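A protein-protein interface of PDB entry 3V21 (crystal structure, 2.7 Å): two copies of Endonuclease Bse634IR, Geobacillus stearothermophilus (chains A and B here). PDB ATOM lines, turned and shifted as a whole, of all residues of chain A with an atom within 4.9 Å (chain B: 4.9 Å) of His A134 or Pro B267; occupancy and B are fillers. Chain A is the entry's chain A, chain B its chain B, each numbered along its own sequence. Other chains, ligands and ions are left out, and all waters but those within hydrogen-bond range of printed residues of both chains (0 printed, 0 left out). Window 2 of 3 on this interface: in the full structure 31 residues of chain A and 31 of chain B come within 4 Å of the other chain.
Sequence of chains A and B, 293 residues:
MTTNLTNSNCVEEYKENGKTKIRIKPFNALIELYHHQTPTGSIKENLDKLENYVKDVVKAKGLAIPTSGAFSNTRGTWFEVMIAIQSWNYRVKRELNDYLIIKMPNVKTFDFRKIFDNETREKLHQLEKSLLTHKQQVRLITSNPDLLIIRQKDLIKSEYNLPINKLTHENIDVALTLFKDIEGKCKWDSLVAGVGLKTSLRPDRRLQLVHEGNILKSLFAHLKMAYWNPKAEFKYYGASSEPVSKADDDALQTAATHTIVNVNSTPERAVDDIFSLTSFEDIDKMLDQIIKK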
ATOM      1  N   SER A 130      11.079  24.414 -17.837  1.00  0.00           N
ATOM      2  CA  SER A 130      11.423  23.171 -18.509  1.00  0.00           C
ATOM      3  C   SER A 130      12.653  22.526 -17.910  1.00  0.00           C
ATOM      4  O   SER A 130      12.637  21.355 -17.558  1.00  0.00           O
ATOM      5  CB  SER A 130      11.646  23.400 -19.996  1.00  0.00           C
ATOM      6  OG  SER A 130      11.892  22.167 -20.635  1.00  0.00           O
ATOM      7  N   LEU A 131      13.721  23.301 -17.789  1.00  0.00           N
ATOM      8  CA  LEU A 131      14.965  22.792 -17.237  1.00  0.00           C
ATOM      9  C   LEU A 131      14.816  22.284 -15.802  1.00  0.00           C
ATOM     10  O   LEU A 131      15.562  21.394 -15.380  1.00  0.00           O
ATOM     11  CB  LEU A 131      16.046  23.873 -17.305  1.00  0.00           C
ATOM     12  CG  LEU A 131      16.408  24.353 -18.712  1.00  0.00           C
ATOM     13  CD1 LEU A 131      17.465  25.432 -18.622  1.00  0.00           C
ATOM     14  CD2 LEU A 131      16.914  23.195 -19.543  1.00  0.00           C
ATOM     15  N   LEU A 132      13.864  22.845 -15.054  1.00  0.00           N
ATOM     16  CA  LEU A 132      13.632  22.427 -13.667  1.00  0.00           C
ATOM     17  C   LEU A 132      12.746  21.182 -13.599  1.00  0.00           C
ATOM     18  O   LEU A 132      12.668  20.509 -12.569  1.00  0.00           O
ATOM     19  CB  LEU A 132      12.977  23.553 -12.871  1.00  0.00           C
ATOM     20  CG  LEU A 132      13.896  24.697 -12.475  1.00  0.00           C
ATOM     21  CD1 LEU A 132      13.057  25.803 -11.876  1.00  0.00           C
ATOM     22  CD2 LEU A 132      14.947  24.212 -11.487  1.00  0.00           C
ATOM     23  N   THR A 133      12.089  20.885 -14.712  1.00  0.00           N
ATOM     24  CA  THR A 133      11.198  19.745 -14.811  1.00  0.00           C
ATOM     25  C   THR A 133      11.965  18.489 -15.205  1.00  0.00           C
ATOM     26  O   THR A 133      11.697  17.882 -16.242  1.00  0.00           O
ATOM     27  CB  THR A 133      10.071  20.034 -15.838  1.00  0.00           C
ATOM     28  OG1 THR A 133       9.276  21.131 -15.368  1.00  0.00           O
ATOM     29  CG2 THR A 133       9.170  18.830 -16.031  1.00  0.00           C
ATOM     30  N   HIS A 134      12.937  18.115 -14.374  1.00  0.00           N
ATOM     31  CA  HIS A 134      13.755  16.913 -14.594  1.00  0.00           C
ATOM     32  C   HIS A 134      14.237  16.320 -13.269  1.00  0.00           C
ATOM     33  O   HIS A 134      14.173  16.975 -12.220  1.00  0.00           O
ATOM     34  CB  HIS A 134      14.991  17.207 -15.448  1.00  0.00           C
ATOM     35  CG  HIS A 134      14.680  17.647 -16.843  1.00  0.00           C
ATOM     36  ND1 HIS A 134      14.625  18.972 -17.207  1.00  0.00           N
ATOM     37  CD2 HIS A 134      14.414  16.932 -17.961  1.00  0.00           C
ATOM     38  CE1 HIS A 134      14.346  19.060 -18.493  1.00  0.00           C
ATOM     39  NE2 HIS A 134      14.207  17.840 -18.975  1.00  0.00           N
ATOM     40  N   LYS A 135      14.744  15.084 -13.342  1.00  0.00           N
ATOM     41  CA  LYS A 135      15.286  14.364 -12.182  1.00  0.00           C
ATOM     42  C   LYS A 135      16.379  15.228 -11.607  1.00  0.00           C
ATOM     43  O   LYS A 135      16.353  15.585 -10.427  1.00  0.00           O
ATOM     44  CB  LYS A 135      15.915  13.043 -12.612  1.00  0.00           C
ATOM     45  CG  LYS A 135      14.934  11.975 -13.067  1.00  0.00           C
ATOM     46  CD  LYS A 135      14.287  11.245 -11.883  1.00  0.00           C
ATOM     47  CE  LYS A 135      13.525  10.000 -12.348  1.00  0.00           C
ATOM     48  NZ  LYS A 135      12.973   9.219 -11.208  1.00  0.00           N
ATOM     49  N   GLN A 136      17.352  15.531 -12.464  1.00  0.00           N
ATOM     50  CA  GLN A 136      18.476  16.386 -12.115  1.00  0.00           C
ATOM     51  C   GLN A 136      18.012  17.771 -12.562  1.00  0.00           C
ATOM     52  O   GLN A 136      18.067  18.082 -13.753  1.00  0.00           O
ATOM     53  CB  GLN A 136      19.735  15.970 -12.901  1.00  0.00           C
ATOM     54  CG  GLN A 136      21.043  16.602 -12.396  1.00  0.00           C
ATOM     55  CD  GLN A 136      22.294  16.222 -13.214  1.00  0.00           C
ATOM     56  OE1 GLN A 136      22.331  16.390 -14.435  1.00  0.00           O
ATOM     57  NE2 GLN A 136      23.329  15.734 -12.525  1.00  0.00           N
ATOM     58  N   GLN A 137      17.512  18.580 -11.624  1.00  0.00           N
ATOM     59  CA  GLN A 137      17.061  19.927 -11.963  1.00  0.00           C
ATOM     60  C   GLN A 137      18.227  20.761 -12.461  1.00  0.00           C
ATOM     61  O   GLN A 137      19.310  20.765 -11.872  1.00  0.00           O
ATOM     62  CB  GLN A 137      16.451  20.628 -10.761  1.00  0.00           C
ATOM     63  CG  GLN A 137      15.135  20.076 -10.321  1.00  0.00           C
ATOM     64  CD  GLN A 137      14.432  21.040  -9.406  1.00  0.00           C
ATOM     65  OE1 GLN A 137      15.039  21.594  -8.483  1.00  0.00           O
ATOM     66  NE2 GLN A 137      13.145  21.256  -9.652  1.00  0.00           N
ATOM     67  N   VAL A 138      17.983  21.485 -13.539  1.00  0.00           N
ATOM     68  CA  VAL A 138      19.006  22.312 -14.145  1.00  0.00           C
ATOM     69  C   VAL A 138      18.566  23.766 -14.246  1.00  0.00           C
ATOM     70  O   VAL A 138      17.379  24.044 -14.409  1.00  0.00           O
ATOM     71  CB  VAL A 138      19.334  21.774 -15.539  1.00  0.00           C
ATOM     72  CG1 VAL A 138      20.080  22.796 -16.336  1.00  0.00           C
ATOM     73  CG2 VAL A 138      20.152  20.522 -15.412  1.00  0.00           C
ATOM     74  N   THR B 259      24.469  20.929 -23.497  1.00  0.00           N
ATOM     75  CA  THR B 259      23.524  19.845 -23.284  1.00  0.00           C
ATOM     76  C   THR B 259      22.080  20.312 -23.317  1.00  0.00           C
ATOM     77  O   THR B 259      21.176  19.507 -23.102  1.00  0.00           O
ATOM     78  CB  THR B 259      23.736  19.155 -21.930  1.00  0.00           C
ATOM     79  OG1 THR B 259      23.323  20.036 -20.873  1.00  0.00           O
ATOM     80  CG2 THR B 259      25.198  18.778 -21.749  1.00  0.00           C
ATOM     81  N   ILE B 260      21.846  21.599 -23.564  1.00  0.00           N
ATOM     82  CA  ILE B 260      20.473  22.099 -23.613  1.00  0.00           C
ATOM     83  C   ILE B 260      20.162  22.806 -24.921  1.00  0.00           C
ATOM     84  O   ILE B 260      19.190  23.544 -25.018  1.00  0.00           O
ATOM     85  CB  ILE B 260      20.178  23.071 -22.468  1.00  0.00           C
ATOM     86  CG1 ILE B 260      21.060  24.313 -22.611  1.00  0.00           C
ATOM     87  CG2 ILE B 260      20.398  22.375 -21.133  1.00  0.00           C
ATOM     88  CD1 ILE B 260      20.704  25.433 -21.653  1.00  0.00           C
ATOM     89  N   SER B 265      17.364  17.366 -26.277  1.00  0.00           N
ATOM     90  CA  SER B 265      18.611  17.100 -25.544  1.00  0.00           C
ATOM     91  C   SER B 265      18.346  17.181 -24.031  1.00  0.00           C
ATOM     92  O   SER B 265      17.838  18.196 -23.540  1.00  0.00           O
ATOM     93  CB  SER B 265      19.695  18.125 -25.956  1.00  0.00           C
ATOM     94  OG  SER B 265      20.984  17.798 -25.451  1.00  0.00           O
ATOM     95  N   THR B 266      18.681  16.110 -23.308  1.00  0.00           N
ATOM     96  CA  THR B 266      18.485  16.044 -21.851  1.00  0.00           C
ATOM     97  C   THR B 266      19.439  16.962 -21.101  1.00  0.00           C
ATOM     98  O   THR B 266      20.653  16.801 -21.154  1.00  0.00           O
ATOM     99  CB  THR B 266      18.686  14.611 -21.301  1.00  0.00           C
ATOM    100  OG1 THR B 266      17.798  13.710 -21.974  1.00  0.00           O
ATOM    101  CG2 THR B 266      18.394  14.565 -19.809  1.00  0.00           C
ATOM    102  N   PRO B 267      18.887  17.922 -20.361  1.00  0.00           N
ATOM    103  CA  PRO B 267      19.706  18.867 -19.604  1.00  0.00           C
ATOM    104  C   PRO B 267      20.679  18.140 -18.711  1.00  0.00           C
ATOM    105  O   PRO B 267      20.388  17.061 -18.212  1.00  0.00           O
ATOM    106  CB  PRO B 267      18.682  19.648 -18.790  1.00  0.00           C
ATOM    107  CG  PRO B 267      17.405  19.471 -19.573  1.00  0.00           C
ATOM    108  CD  PRO B 267      17.474  18.033 -19.976  1.00  0.00           C
ATOM    109  N   GLU B 268      21.837  18.744 -18.514  1.00  0.00           N
ATOM    110  CA  GLU B 268      22.850  18.166 -17.664  1.00  0.00           C
ATOM    111  C   GLU B 268      23.515  19.314 -16.964  1.00  0.00           C
ATOM    112  O   GLU B 268      23.695  20.382 -17.554  1.00  0.00           O
ATOM    113  CB  GLU B 268      23.886  17.420 -18.485  1.00  0.00           C
ATOM    114  CG  GLU B 268      24.832  16.600 -17.643  1.00  0.00           C
ATOM    115  CD  GLU B 268      25.989  16.083 -18.456  1.00  0.00           C
ATOM    116  OE1 GLU B 268      25.792  15.809 -19.665  1.00  0.00           O
ATOM    117  OE2 GLU B 268      27.095  15.946 -17.887  1.00  0.00           O
ATOM    118  N   ARG B 269      23.899  19.091 -15.716  1.00  0.00           N
ATOM    119  CA  ARG B 269      24.536  20.133 -14.927  1.00  0.00           C
ATOM    120  C   ARG B 269      26.023  20.162 -15.121  1.00  0.00           C
ATOM    121  O   ARG B 269      26.645  19.121 -15.296  1.00  0.00           O
ATOM    122  CB  ARG B 269      24.228  19.925 -13.458  1.00  0.00           C
ATOM    123  CG  ARG B 269      22.762  20.084 -13.172  1.00  0.00           C
ATOM    124  CD  ARG B 269      22.394  19.526 -11.826  1.00  0.00           C
ATOM    125  NE  ARG B 269      23.282  19.984 -10.779  1.00  0.00           N
ATOM    126  CZ  ARG B 269      22.971  19.923  -9.492  1.00  0.00           C
ATOM    127  NH1 ARG B 269      21.791  19.422  -9.133  1.00  0.00           N
ATOM    128  NH2 ARG B 269      23.830  20.363  -8.572  1.00  0.00           N
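The side-chain amide oxygen (OE1) of Gln A136 sits at hydrogen-bond distance from the backbone NH (N) of Arg B269 (3.4 Å).
OG1 of Thr B259 is in hydrogen-bond range of N of Glu B268, 3.1 Å away.
NE2 of Gln A137 lies within hydrogen-bond range of O of Leu A132.
A ring nitrogen (ND1) of His A134 lies close to the backbone carbonyl oxygen (O) of Ser A130, at 3.1 Å.
O of Leu A131 sits at hydrogen-bond distance from ND1 of His A134.
The backbone NH (N) of Val A138 is in hydrogen-bond range of the backbone carbonyl oxygen (O) of Leu A131, at 3.0 Å.
Among the printed residues, merely in contact across the chains: Leu A131 with Ile B260 (3.9 Å), Leu A131 with Pro B267 (3.8 Å), His A134 with Pro B267 (3.3 Å), Gln A136 with Glu B268 (3.7 Å), Gln A137 with Arg B269 (3.3 Å), Val A138 with Pro B267 (3.8 Å), Val A138 with Glu B268 (3.9 Å) and Val A138 with Arg B269 (3.5 Å).
Ser A130 touches none of the printed residues of chain B.
Of the printed residues of chain B, Leu A131 touches Ile B260 (3.9 Å) and Pro B267 (3.8 Å).
Printed residues of chain B within 4 Å of His A134: Pro B267 (3.3 Å).
Of the printed residues of chain B, Gln A136 touches Glu B268 (3.7 Å) and Arg B269 (3.3 Å).
Of the printed residues of chain A, Ile B260 touches Leu A131.
Ser B265 touches none of the printed residues of chain A.
Of chain A, only Leu A131 (3.8 Å), His A134 (3.3 Å) and Val A138 (3.8 Å) come within 4 Å of Pro B267.
Of the printed residues of chain A, Arg B269 touches Gln A136, Gln A137 and Val A138.
The nearest residue of chain A that does not touch Pro B267 is Gln A136 (4.3 Å).
Of the 9 printed residues of chain A, 5 touch a printed residue of chain B.
Hydrophobic or aromatic side chains of chain A within 4 Å of the printed part of chain B: Leu A131, His A134 and Val A138.
Of the 7 printed residues of chain B, 4 touch a printed residue of chain A.
Printed residues of chain B that touch a printed residue of chain A: Ile B260, Pro B267, Glu B268 and Arg B269.
Hydrophobic or aromatic side chains of chain B within 4 Å of the printed part of chain A: Ile B260 and Pro B267.
Among the printed residues, 9 pairs touch across the chains.
No position is printed for both chains.
Of the 9 pairs that touch across the chains among the printed residues, none has its exchanged pair printed and touching as well.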
